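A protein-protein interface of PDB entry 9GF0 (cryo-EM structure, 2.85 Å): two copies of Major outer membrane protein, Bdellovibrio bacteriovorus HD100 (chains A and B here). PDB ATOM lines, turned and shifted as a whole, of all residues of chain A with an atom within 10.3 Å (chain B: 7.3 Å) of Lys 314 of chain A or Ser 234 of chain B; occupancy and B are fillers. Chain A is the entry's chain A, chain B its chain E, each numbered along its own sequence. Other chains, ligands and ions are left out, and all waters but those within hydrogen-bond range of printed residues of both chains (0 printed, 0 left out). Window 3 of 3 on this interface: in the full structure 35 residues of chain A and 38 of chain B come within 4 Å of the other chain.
The side-chain amino group (NZ) of Lys 54 of chain A lies within hydrogen-bond range of the backbone carbonyl oxygen (O) of Leu 231 of chain B, 3.3 Å away. The side-chain hydroxyl (OG) of Ser 315 of chain A is in hydrogen-bond range of a ring nitrogen (ND1) of His 267 of chain B (3.0 Å). O of Gly 237 of chain B sits at hydrogen-bond distance from OH of Tyr 342 of chain A (3.5 Å). O of Phe 312 of chain A sits close to O of Ala 269 of chain B (3.4 Å).
The backbone carbonyl oxygen of Glu 32 of chain A sits at hydrogen-bond distance from the backbone NH of Phe 344 of chain A (3.2 Å). The backbone carbonyl oxygen (O) of Tyr 340 of chain A sits close to the side-chain hydroxyl (OG1) of Thr 35 of chain A (3.4 Å). O of Lys 314 of chain A is in hydrogen-bond range of N of Thr 343 of chain A, 2.9 Å away. The backbone carbonyl oxygen (O) of Phe 239 of chain B sits at hydrogen-bond distance from the backbone NH (N) of Leu 231 of chain B (3.0 Å). The backbone carbonyl oxygen of Ala 232 of chain B lies close to the side-chain amide oxygen of Asn 238 of chain B (2.8 Å). NE2 of His 267 of chain B lies within hydrogen-bond range of OE2 of Glu 236 of chain B (3.0 Å).
Among the printed residues, merely in contact across the chains: Ala 34 of chain A with Phe 239 of chain B, Lys 314 of chain A with Ser 234 of chain B, Lys 314 of chain A with His 267 of chain B, Tyr 340 of chain A with His 267 of chain B, Tyr 342 of chain A with His 267 of chain B, Phe 344 of chain A with Leu 231 of chain B, Phe 344 of chain A with Ala 232 of chain B and Phe 344 of chain A with Phe 239 of chain B.
Of the printed residues of chain B, Ala 34 of chain A touches Phe 239 (3.5 Å). Of chain B, only Ser 234 and His 267 come within 4 Å of Lys 314 of chain A. Of chain A, only Phe 344 (3.8 Å) comes within 4 Å of Ala 232 of chain B. Of the printed residues of chain A, Ser 234 of chain B touches Lys 314 (3.9 Å). Gly 237 of chain B touches just one residue of chain A: Tyr 342. Of the printed residues of chain A, Phe 239 of chain B touches Ala 34 and Phe 344. Of the printed residues of chain A, His 267 of chain B touches Lys 314, Ser 315, Tyr 340 and Tyr 342. The nearest residue of chain B that does not touch Lys 314 of chain A is Glu 236 of chain B (4.1 Å). The nearest printed residue of chain A that does not touch Ser 234 of chain B is Tyr 342 of chain A (4.02 Å).
Printed residues of chain B that touch a printed residue of chain A: Leu 231, Ala 232, Ser 234, Gly 237, Phe 239, His 267 and Ala 269. Of the 23 printed residues of chain A, 8 touch a printed residue of chain B. Printed residues of chain A that touch a printed residue of chain B: Ala 34, Lys 54, Phe 312, Lys 314, Ser 315, Tyr 340, Tyr 342 and Phe 344. Hydrophobic or aromatic side chains of chain A within 4 Å of the printed part of chain B: Ala 34, Phe 312, Tyr 340, Tyr 342 and Phe 344. Among the printed residues, 12 pairs touch across the chains. Among the printed residues, no Asp or Glu carboxylate lies within 4 Å of a Lys or Arg side-chain nitrogen of the other chain.
No position is printed for both chains. Of the 12 pairs that touch across the chains among the printed residues, none has its exchanged pair printed and touching as well.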
ATOM      1  N   SER A  31      -8.752 -25.658  17.870  1.00  0.00           N
ATOM      2  CA  SER A  31      -9.593 -24.525  17.535  1.00  0.00           C
ATOM      3  C   SER A  31     -11.047 -24.841  17.868  1.00  0.00           C
ATOM      4  O   SER A  31     -11.454 -26.003  17.942  1.00  0.00           O
ATOM      5  CB  SER A  31      -9.460 -24.174  16.057  1.00  0.00           C
ATOM      6  OG  SER A  31      -9.472 -25.347  15.265  1.00  0.00           O
ATOM      7  N   GLU A  32     -11.832 -23.790  18.082  1.00  0.00           N
ATOM      8  CA  GLU A  32     -13.252 -23.970  18.345  1.00  0.00           C
ATOM      9  C   GLU A  32     -13.934 -24.596  17.138  1.00  0.00           C
ATOM     10  O   GLU A  32     -13.757 -24.139  16.006  1.00  0.00           O
ATOM     11  CB  GLU A  32     -13.894 -22.630  18.681  1.00  0.00           C
ATOM     12  CG  GLU A  32     -13.881 -22.307  20.149  1.00  0.00           C
ATOM     13  CD  GLU A  32     -14.325 -20.893  20.426  1.00  0.00           C
ATOM     14  OE1 GLU A  32     -14.308 -20.074  19.485  1.00  0.00           O
ATOM     15  OE2 GLU A  32     -14.687 -20.598  21.583  1.00  0.00           O
ATOM     16  N   GLN A  33     -14.724 -25.638  17.378  1.00  0.00           N
ATOM     17  CA  GLN A  33     -15.294 -26.411  16.284  1.00  0.00           C
ATOM     18  C   GLN A  33     -16.381 -27.321  16.830  1.00  0.00           C
ATOM     19  O   GLN A  33     -16.520 -27.502  18.041  1.00  0.00           O
ATOM     20  CB  GLN A  33     -14.224 -27.238  15.574  1.00  0.00           C
ATOM     21  CG  GLN A  33     -13.868 -28.516  16.308  1.00  0.00           C
ATOM     22  CD  GLN A  33     -12.467 -28.972  16.021  1.00  0.00           C
ATOM     23  OE1 GLN A  33     -11.564 -28.773  16.827  1.00  0.00           O
ATOM     24  NE2 GLN A  33     -12.269 -29.580  14.862  1.00  0.00           N
ATOM     25  N   ALA A  34     -17.153 -27.893  15.906  1.00  0.00           N
ATOM     26  CA  ALA A  34     -18.118 -28.944  16.192  1.00  0.00           C
ATOM     27  C   ALA A  34     -18.080 -29.948  15.053  1.00  0.00           C
ATOM     28  O   ALA A  34     -17.991 -29.564  13.885  1.00  0.00           O
ATOM     29  CB  ALA A  34     -19.532 -28.391  16.360  1.00  0.00           C
ATOM     30  N   THR A  35     -18.140 -31.231  15.394  1.00  0.00           N
ATOM     31  CA  THR A  35     -17.968 -32.299  14.421  1.00  0.00           C
ATOM     32  C   THR A  35     -19.082 -33.324  14.566  1.00  0.00           C
ATOM     33  O   THR A  35     -19.488 -33.653  15.683  1.00  0.00           O
ATOM     34  CB  THR A  35     -16.598 -32.979  14.586  1.00  0.00           C
ATOM     35  OG1 THR A  35     -16.550 -34.173  13.798  1.00  0.00           O
ATOM     36  CG2 THR A  35     -16.343 -33.327  16.037  1.00  0.00           C
ATOM     37  N   LYS A  54     -15.716 -25.353  22.834  1.00  0.00           N
ATOM     38  CA  LYS A  54     -15.800 -23.868  22.829  1.00  0.00           C
ATOM     39  C   LYS A  54     -14.887 -23.296  23.919  1.00  0.00           C
ATOM     40  O   LYS A  54     -14.679 -23.987  24.929  1.00  0.00           O
ATOM     41  CB  LYS A  54     -17.249 -23.425  23.045  1.00  0.00           C
ATOM     42  CG  LYS A  54     -17.485 -21.922  22.991  1.00  0.00           C
ATOM     43  CD  LYS A  54     -18.938 -21.536  23.162  1.00  0.00           C
ATOM     44  CE  LYS A  54     -19.165 -20.039  23.132  1.00  0.00           C
ATOM     45  NZ  LYS A  54     -20.597 -19.697  23.301  1.00  0.00           N
ATOM     46  N   SER A 271      -6.957 -25.625  -2.808  1.00  0.00           N
ATOM     47  CA  SER A 271      -7.704 -24.830  -1.843  1.00  0.00           C
ATOM     48  C   SER A 271      -8.967 -25.527  -1.366  1.00  0.00           C
ATOM     49  O   SER A 271      -9.560 -25.087  -0.379  1.00  0.00           O
ATOM     50  CB  SER A 271      -8.064 -23.472  -2.439  1.00  0.00           C
ATOM     51  OG  SER A 271      -9.149 -23.583  -3.339  1.00  0.00           O
ATOM     52  N   TRP A 272      -9.386 -26.597  -2.035  1.00  0.00           N
ATOM     53  CA  TRP A 272     -10.573 -27.347  -1.662  1.00  0.00           C
ATOM     54  C   TRP A 272     -10.273 -28.787  -1.277  1.00  0.00           C
ATOM     55  O   TRP A 272     -11.202 -29.524  -0.937  1.00  0.00           O
ATOM     56  CB  TRP A 272     -11.591 -27.332  -2.812  1.00  0.00           C
ATOM     57  CG  TRP A 272     -11.062 -27.881  -4.104  1.00  0.00           C
ATOM     58  CD1 TRP A 272     -10.369 -27.204  -5.057  1.00  0.00           C
ATOM     59  CD2 TRP A 272     -11.197 -29.221  -4.584  1.00  0.00           C
ATOM     60  NE1 TRP A 272     -10.054 -28.038  -6.097  1.00  0.00           N
ATOM     61  CE2 TRP A 272     -10.551 -29.284  -5.829  1.00  0.00           C
ATOM     62  CE3 TRP A 272     -11.794 -30.376  -4.078  1.00  0.00           C
ATOM     63  CZ2 TRP A 272     -10.488 -30.452  -6.574  1.00  0.00           C
ATOM     64  CZ3 TRP A 272     -11.728 -31.533  -4.818  1.00  0.00           C
ATOM     65  CH2 TRP A 272     -11.081 -31.564  -6.052  1.00  0.00           C
ATOM     66  N   ILE A 310     -12.471 -32.516   2.043  1.00  0.00           N
ATOM     67  CA  ILE A 310     -12.981 -31.478   1.154  1.00  0.00           C
ATOM     68  C   ILE A 310     -13.270 -30.231   1.978  1.00  0.00           C
ATOM     69  O   ILE A 310     -14.142 -30.242   2.851  1.00  0.00           O
ATOM     70  CB  ILE A 310     -14.239 -31.952   0.410  1.00  0.00           C
ATOM     71  CG1 ILE A 310     -14.072 -33.398  -0.060  1.00  0.00           C
ATOM     72  CG2 ILE A 310     -14.540 -31.039  -0.757  1.00  0.00           C
ATOM     73  CD1 ILE A 310     -13.309 -33.543  -1.347  1.00  0.00           C
ATOM     74  N   LYS A 311     -12.548 -29.153   1.689  1.00  0.00           N
ATOM     75  CA  LYS A 311     -12.656 -27.904   2.431  1.00  0.00           C
ATOM     76  C   LYS A 311     -13.607 -26.956   1.722  1.00  0.00           C
ATOM     77  O   LYS A 311     -13.498 -26.747   0.510  1.00  0.00           O
ATOM     78  CB  LYS A 311     -11.291 -27.234   2.591  1.00  0.00           C
ATOM     79  CG  LYS A 311     -10.232 -28.090   3.240  1.00  0.00           C
ATOM     80  CD  LYS A 311      -8.946 -28.013   2.459  1.00  0.00           C
ATOM     81  CE  LYS A 311      -8.155 -26.769   2.795  1.00  0.00           C
ATOM     82  NZ  LYS A 311      -6.876 -26.713   2.038  1.00  0.00           N
ATOM     83  N   PHE A 312     -14.534 -26.385   2.483  1.00  0.00           N
ATOM     84  CA  PHE A 312     -15.476 -25.386   2.000  1.00  0.00           C
ATOM     85  C   PHE A 312     -15.411 -24.135   2.862  1.00  0.00           C
ATOM     86  O   PHE A 312     -16.425 -23.502   3.144  1.00  0.00           O
ATOM     87  CB  PHE A 312     -16.895 -25.945   1.974  1.00  0.00           C
ATOM     88  CG  PHE A 312     -17.164 -26.866   0.825  1.00  0.00           C
ATOM     89  CD1 PHE A 312     -17.079 -26.412  -0.476  1.00  0.00           C
ATOM     90  CD2 PHE A 312     -17.505 -28.186   1.047  1.00  0.00           C
ATOM     91  CE1 PHE A 312     -17.323 -27.255  -1.529  1.00  0.00           C
ATOM     92  CE2 PHE A 312     -17.751 -29.030  -0.006  1.00  0.00           C
ATOM     93  CZ  PHE A 312     -17.662 -28.564  -1.295  1.00  0.00           C
ATOM     94  N   GLY A 313     -14.214 -23.765   3.296  1.00  0.00           N
ATOM     95  CA  GLY A 313     -14.071 -22.637   4.192  1.00  0.00           C
ATOM     96  C   GLY A 313     -14.077 -23.049   5.647  1.00  0.00           C
ATOM     97  O   GLY A 313     -13.070 -23.550   6.154  1.00  0.00           O
ATOM     98  N   LYS A 314     -15.197 -22.846   6.334  1.00  0.00           N
ATOM     99  CA  LYS A 314     -15.337 -23.278   7.715  1.00  0.00           C
ATOM    100  C   LYS A 314     -15.906 -24.684   7.845  1.00  0.00           C
ATOM    101  O   LYS A 314     -15.965 -25.210   8.958  1.00  0.00           O
ATOM    102  CB  LYS A 314     -16.218 -22.300   8.493  1.00  0.00           C
ATOM    103  CG  LYS A 314     -15.917 -20.846   8.218  1.00  0.00           C
ATOM    104  CD  LYS A 314     -17.010 -19.942   8.752  1.00  0.00           C
ATOM    105  CE  LYS A 314     -17.379 -20.308  10.169  1.00  0.00           C
ATOM    106  NZ  LYS A 314     -17.140 -19.180  11.104  1.00  0.00           N
ATOM    107  N   SER A 315     -16.314 -25.304   6.744  1.00  0.00           N
ATOM    108  CA  SER A 315     -16.871 -26.648   6.752  1.00  0.00           C
ATOM    109  C   SER A 315     -15.927 -27.570   5.999  1.00  0.00           C
ATOM    110  O   SER A 315     -15.489 -27.243   4.892  1.00  0.00           O
ATOM    111  CB  SER A 315     -18.260 -26.677   6.112  1.00  0.00           C
ATOM    112  OG  SER A 315     -19.257 -26.278   7.033  1.00  0.00           O
ATOM    113  N   VAL A 316     -15.606 -28.713   6.601  1.00  0.00           N
ATOM    114  CA  VAL A 316     -14.690 -29.681   6.014  1.00  0.00           C
ATOM    115  C   VAL A 316     -15.334 -31.056   6.083  1.00  0.00           C
ATOM    116  O   VAL A 316     -15.759 -31.495   7.156  1.00  0.00           O
ATOM    117  CB  VAL A 316     -13.323 -29.680   6.725  1.00  0.00           C
ATOM    118  CG1 VAL A 316     -12.407 -30.718   6.111  1.00  0.00           C
ATOM    119  CG2 VAL A 316     -12.685 -28.309   6.642  1.00  0.00           C
ATOM    120  N   ILE A 317     -15.398 -31.735   4.942  1.00  0.00           N
ATOM    121  CA  ILE A 317     -15.985 -33.066   4.842  1.00  0.00           C
ATOM    122  C   ILE A 317     -14.825 -34.052   4.760  1.00  0.00           C
ATOM    123  O   ILE A 317     -14.267 -34.283   3.686  1.00  0.00           O
ATOM    124  CB  ILE A 317     -16.912 -33.189   3.630  1.00  0.00           C
ATOM    125  CG1 ILE A 317     -18.087 -32.211   3.733  1.00  0.00           C
ATOM    126  CG2 ILE A 317     -17.427 -34.617   3.506  1.00  0.00           C
ATOM    127  CD1 ILE A 317     -19.356 -32.807   4.282  1.00  0.00           C
ATOM    128  N   ASP A 318     -14.453 -34.636   5.894  1.00  0.00           N
ATOM    129  CA  ASP A 318     -13.376 -35.614   5.934  1.00  0.00           C
ATOM    130  C   ASP A 318     -13.906 -36.997   5.581  1.00  0.00           C
ATOM    131  O   ASP A 318     -14.947 -37.426   6.082  1.00  0.00           O
ATOM    132  CB  ASP A 318     -12.718 -35.645   7.312  1.00  0.00           C
ATOM    133  CG  ASP A 318     -11.888 -34.409   7.597  1.00  0.00           C
ATOM    134  OD1 ASP A 318     -11.129 -33.973   6.709  1.00  0.00           O
ATOM    135  OD2 ASP A 318     -11.987 -33.877   8.722  1.00  0.00           O
ATOM    136  N   ALA A 339     -17.328 -37.790   7.776  1.00  0.00           N
ATOM    137  CA  ALA A 339     -17.642 -36.955   8.922  1.00  0.00           C
ATOM    138  C   ALA A 339     -17.715 -35.508   8.464  1.00  0.00           C
ATOM    139  O   ALA A 339     -17.185 -35.141   7.414  1.00  0.00           O
ATOM    140  CB  ALA A 339     -16.606 -37.101  10.037  1.00  0.00           C
ATOM    141  N   TYR A 340     -18.388 -34.687   9.260  1.00  0.00           N
ATOM    142  CA  TYR A 340     -18.562 -33.271   8.971  1.00  0.00           C
ATOM    143  C   TYR A 340     -18.067 -32.467  10.162  1.00  0.00           C
ATOM    144  O   TYR A 340     -18.401 -32.782  11.306  1.00  0.00           O
ATOM    145  CB  TYR A 340     -20.031 -32.955   8.674  1.00  0.00           C
ATOM    146  CG  TYR A 340     -20.327 -31.509   8.368  1.00  0.00           C
ATOM    147  CD1 TYR A 340     -19.964 -30.952   7.160  1.00  0.00           C
ATOM    148  CD2 TYR A 340     -20.989 -30.710   9.285  1.00  0.00           C
ATOM    149  CE1 TYR A 340     -20.240 -29.642   6.873  1.00  0.00           C
ATOM    150  CE2 TYR A 340     -21.269 -29.396   9.007  1.00  0.00           C
ATOM    151  CZ  TYR A 340     -20.892 -28.867   7.797  1.00  0.00           C
ATOM    152  OH  TYR A 340     -21.165 -27.553   7.505  1.00  0.00           O
ATOM    153  N   THR A 341     -17.257 -31.448   9.894  1.00  0.00           N
ATOM    154  CA  THR A 341     -16.710 -30.582  10.928  1.00  0.00           C
ATOM    155  C   THR A 341     -16.973 -29.136  10.545  1.00  0.00           C
ATOM    156  O   THR A 341     -16.683 -28.727   9.418  1.00  0.00           O
ATOM    157  CB  THR A 341     -15.205 -30.818  11.120  1.00  0.00           C
ATOM    158  OG1 THR A 341     -14.999 -31.981  11.929  1.00  0.00           O
ATOM    159  CG2 THR A 341     -14.551 -29.634  11.799  1.00  0.00           C
ATOM    160  N   TYR A 342     -17.528 -28.368  11.477  1.00  0.00           N
ATOM    161  CA  TYR A 342     -17.772 -26.944  11.288  1.00  0.00           C
ATOM    162  C   TYR A 342     -16.933 -26.189  12.308  1.00  0.00           C
ATOM    163  O   TYR A 342     -17.168 -26.300  13.515  1.00  0.00           O
ATOM    164  CB  TYR A 342     -19.253 -26.614  11.441  1.00  0.00           C
ATOM    165  CG  TYR A 342     -19.570 -25.145  11.338  1.00  0.00           C
ATOM    166  CD1 TYR A 342     -19.597 -24.507  10.112  1.00  0.00           C
ATOM    167  CD2 TYR A 342     -19.855 -24.399  12.467  1.00  0.00           C
ATOM    168  CE1 TYR A 342     -19.889 -23.173  10.015  1.00  0.00           C
ATOM    169  CE2 TYR A 342     -20.149 -23.062  12.377  1.00  0.00           C
ATOM    170  CZ  TYR A 342     -20.165 -22.457  11.149  1.00  0.00           C
ATOM    171  OH  TYR A 342     -20.458 -21.120  11.059  1.00  0.00           O
ATOM    172  N   THR A 343     -15.958 -25.430  11.826  1.00  0.00           N
ATOM    173  CA  THR A 343     -15.077 -24.662  12.691  1.00  0.00           C
ATOM    174  C   THR A 343     -15.621 -23.248  12.818  1.00  0.00           C
ATOM    175  O   THR A 343     -15.994 -22.619  11.827  1.00  0.00           O
ATOM    176  CB  THR A 343     -13.650 -24.648  12.145  1.00  0.00           C
ATOM    177  OG1 THR A 343     -13.011 -25.892  12.451  1.00  0.00           O
ATOM    178  CG2 THR A 343     -12.852 -23.527  12.769  1.00  0.00           C
ATOM    179  N   PHE A 344     -15.936 -22.897  14.064  1.00  0.00           N
ATOM    180  CA  PHE A 344     -16.563 -21.589  14.343  1.00  0.00           C
ATOM    181  C   PHE A 344     -15.616 -20.481  13.893  1.00  0.00           C
ATOM    182  O   PHE A 344     -15.545 -19.482  14.640  1.00  0.00           O
ATOM    183  CB  PHE A 344     -16.854 -21.450  15.838  1.00  0.00           C
ATOM    184  CG  PHE A 344     -17.623 -22.572  16.486  1.00  0.00           C
ATOM    185  CD1 PHE A 344     -18.462 -23.390  15.750  1.00  0.00           C
ATOM    186  CD2 PHE A 344     -17.518 -22.796  17.849  1.00  0.00           C
ATOM    187  CE1 PHE A 344     -19.164 -24.415  16.361  1.00  0.00           C
ATOM    188  CE2 PHE A 344     -18.222 -23.820  18.459  1.00  0.00           C
ATOM    189  CZ  PHE A 344     -19.046 -24.625  17.714  1.00  0.00           C
ATOM    190  OXT PHE A 344     -14.972 -20.587  12.849  1.00  0.00           O
ATOM    191  N   GLU B 195     -31.991 -14.771  19.550  1.00  0.00           N
ATOM    192  CA  GLU B 195     -31.151 -15.961  19.551  1.00  0.00           C
ATOM    193  C   GLU B 195     -31.746 -17.110  20.348  1.00  0.00           C
ATOM    194  O   GLU B 195     -31.578 -18.268  19.965  1.00  0.00           O
ATOM    195  CB  GLU B 195     -29.761 -15.618  20.110  1.00  0.00           C
ATOM    196  CG  GLU B 195     -28.659 -15.545  19.063  1.00  0.00           C
ATOM    197  CD  GLU B 195     -28.682 -14.254  18.265  1.00  0.00           C
ATOM    198  OE1 GLU B 195     -28.826 -13.175  18.875  1.00  0.00           O
ATOM    199  OE2 GLU B 195     -28.546 -14.320  17.026  1.00  0.00           O
ATOM    200  N   THR B 230     -28.246 -20.360  20.379  1.00  0.00           N
ATOM    201  CA  THR B 230     -27.135 -20.399  19.392  1.00  0.00           C
ATOM    202  C   THR B 230     -25.795 -20.462  20.134  1.00  0.00           C
ATOM    203  O   THR B 230     -25.555 -19.569  20.964  1.00  0.00           O
ATOM    204  CB  THR B 230     -27.146 -19.166  18.483  1.00  0.00           C
ATOM    205  OG1 THR B 230     -26.563 -18.079  19.201  1.00  0.00           O
ATOM    206  CG2 THR B 230     -28.536 -18.796  18.018  1.00  0.00           C
ATOM    207  N   LEU B 231     -24.964 -21.474  19.854  1.00  0.00           N
ATOM    208  CA  LEU B 231     -23.615 -21.577  20.470  1.00  0.00           C
ATOM    209  C   LEU B 231     -22.670 -20.655  19.698  1.00  0.00           C
ATOM    210  O   LEU B 231     -22.063 -19.770  20.328  1.00  0.00           O
ATOM    211  CB  LEU B 231     -23.141 -23.032  20.394  1.00  0.00           C
ATOM    212  CG  LEU B 231     -21.735 -23.319  20.918  1.00  0.00           C
ATOM    213  CD1 LEU B 231     -21.645 -23.011  22.402  1.00  0.00           C
ATOM    214  CD2 LEU B 231     -21.367 -24.769  20.662  1.00  0.00           C
ATOM    215  N   ALA B 232     -22.556 -20.861  18.385  1.00  0.00           N
ATOM    216  CA  ALA B 232     -21.724 -19.973  17.543  1.00  0.00           C
ATOM    217  C   ALA B 232     -22.616 -18.880  16.954  1.00  0.00           C
ATOM    218  O   ALA B 232     -23.624 -19.228  16.331  1.00  0.00           O
ATOM    219  CB  ALA B 232     -21.065 -20.777  16.456  1.00  0.00           C
ATOM    220  N   LYS B 233     -22.302 -17.612  17.206  1.00  0.00           N
ATOM    221  CA  LYS B 233     -23.095 -16.495  16.631  1.00  0.00           C
ATOM    222  C   LYS B 233     -22.308 -15.957  15.440  1.00  0.00           C
ATOM    223  O   LYS B 233     -21.423 -15.112  15.654  1.00  0.00           O
ATOM    224  CB  LYS B 233     -23.356 -15.409  17.679  1.00  0.00           C
ATOM    225  CG  LYS B 233     -24.267 -15.820  18.828  1.00  0.00           C
ATOM    226  CD  LYS B 233     -24.475 -14.721  19.849  1.00  0.00           C
ATOM    227  CE  LYS B 233     -25.398 -15.124  20.978  1.00  0.00           C
ATOM    228  NZ  LYS B 233     -25.564 -14.036  21.972  1.00  0.00           N
ATOM    229  N   SER B 234     -22.615 -16.432  14.232  1.00  0.00           N
ATOM    230  CA  SER B 234     -21.792 -16.035  13.063  1.00  0.00           C
ATOM    231  C   SER B 234     -22.629 -15.883  11.798  1.00  0.00           C
ATOM    232  O   SER B 234     -23.817 -16.235  11.825  1.00  0.00           O
ATOM    233  CB  SER B 234     -20.712 -17.047  12.825  1.00  0.00           C
ATOM    234  OG  SER B 234     -20.384 -17.122  11.447  1.00  0.00           O
ATOM    235  N   GLU B 235     -22.026 -15.342  10.743  1.00  0.00           N
ATOM    236  CA  GLU B 235     -22.727 -15.276   9.437  1.00  0.00           C
ATOM    237  C   GLU B 235     -22.270 -16.511   8.660  1.00  0.00           C
ATOM    238  O   GLU B 235     -21.553 -17.330   9.266  1.00  0.00           O
ATOM    239  CB  GLU B 235     -22.430 -13.964   8.708  1.00  0.00           C
ATOM    240  CG  GLU B 235     -23.187 -13.827   7.400  1.00  0.00           C
ATOM    241  CD  GLU B 235     -22.962 -12.519   6.661  1.00  0.00           C
ATOM    242  OE1 GLU B 235     -22.165 -11.693   7.149  1.00  0.00           O
ATOM    243  OE2 GLU B 235     -23.586 -12.329   5.598  1.00  0.00           O
ATOM    244  N   GLU B 236     -22.676 -16.644   7.395  1.00  0.00           N
ATOM    245  CA  GLU B 236     -22.359 -17.876   6.629  1.00  0.00           C
ATOM    246  C   GLU B 236     -23.198 -19.013   7.221  1.00  0.00           C
ATOM    247  O   GLU B 236     -23.802 -19.766   6.445  1.00  0.00           O
ATOM    248  CB  GLU B 236     -20.856 -18.157   6.666  1.00  0.00           C
ATOM    249  CG  GLU B 236     -20.063 -17.337   5.672  1.00  0.00           C
ATOM    250  CD  GLU B 236     -19.307 -18.165   4.650  1.00  0.00           C
ATOM    251  OE1 GLU B 236     -19.496 -17.924   3.441  1.00  0.00           O
ATOM    252  OE2 GLU B 236     -18.534 -19.048   5.067  1.00  0.00           O
ATOM    253  N   GLY B 237     -23.231 -19.119   8.549  1.00  0.00           N
ATOM    254  CA  GLY B 237     -24.059 -20.138   9.219  1.00  0.00           C
ATOM    255  C   GLY B 237     -24.168 -19.894  10.708  1.00  0.00           C
ATOM    256  O   GLY B 237     -23.329 -19.164  11.242  1.00  0.00           O
ATOM    257  N   ASN B 238     -25.184 -20.483  11.348  1.00  0.00           N
ATOM    258  CA  ASN B 238     -25.282 -20.391  12.823  1.00  0.00           C
ATOM    259  C   ASN B 238     -25.272 -21.811  13.383  1.00  0.00           C
ATOM    260  O   ASN B 238     -25.964 -22.662  12.816  1.00  0.00           O
ATOM    261  CB  ASN B 238     -26.538 -19.650  13.278  1.00  0.00           C
ATOM    262  CG  ASN B 238     -26.258 -18.520  14.245  1.00  0.00           C
ATOM    263  OD1 ASN B 238     -26.220 -18.731  15.453  1.00  0.00           O
ATOM    264  ND2 ASN B 238     -26.081 -17.314  13.730  1.00  0.00           N
ATOM    265  N   PHE B 239     -24.480 -22.052  14.432  1.00  0.00           N
ATOM    266  CA  PHE B 239     -24.471 -23.369  15.089  1.00  0.00           C
ATOM    267  C   PHE B 239     -25.564 -23.281  16.144  1.00  0.00           C
ATOM    268  O   PHE B 239     -25.430 -22.464  17.049  1.00  0.00           O
ATOM    269  CB  PHE B 239     -23.107 -23.650  15.705  1.00  0.00           C
ATOM    270  CG  PHE B 239     -23.015 -24.941  16.471  1.00  0.00           C
ATOM    271  CD1 PHE B 239     -22.985 -26.153  15.807  1.00  0.00           C
ATOM    272  CD2 PHE B 239     -22.960 -24.938  17.853  1.00  0.00           C
ATOM    273  CE1 PHE B 239     -22.909 -27.339  16.514  1.00  0.00           C
ATOM    274  CE2 PHE B 239     -22.880 -26.125  18.557  1.00  0.00           C
ATOM    275  CZ  PHE B 239     -22.855 -27.320  17.885  1.00  0.00           C
ATOM    276  N   HIS B 267     -24.931 -24.107   6.865  1.00  0.00           N
ATOM    277  CA  HIS B 267     -23.812 -23.246   6.412  1.00  0.00           C
ATOM    278  C   HIS B 267     -23.843 -22.999   4.906  1.00  0.00           C
ATOM    279  O   HIS B 267     -24.070 -23.945   4.142  1.00  0.00           O
ATOM    280  CB  HIS B 267     -22.477 -23.889   6.803  1.00  0.00           C
ATOM    281  CG  HIS B 267     -21.274 -23.041   6.563  1.00  0.00           C
ATOM    282  ND1 HIS B 267     -20.115 -23.538   6.015  1.00  0.00           N
ATOM    283  CD2 HIS B 267     -21.048 -21.748   6.791  1.00  0.00           C
ATOM    284  CE1 HIS B 267     -19.228 -22.565   5.915  1.00  0.00           C
ATOM    285  NE2 HIS B 267     -19.774 -21.470   6.381  1.00  0.00           N
ATOM    286  N   ALA B 269     -21.768 -23.056   2.435  1.00  0.00           N
ATOM    287  CA  ALA B 269     -20.391 -23.499   2.140  1.00  0.00           C
ATOM    288  C   ALA B 269     -19.855 -22.737   0.939  1.00  0.00           C
ATOM    289  O   ALA B 269     -18.802 -22.121   1.088  1.00  0.00           O
ATOM    290  CB  ALA B 269     -20.424 -24.968   1.891  1.00  0.00           C
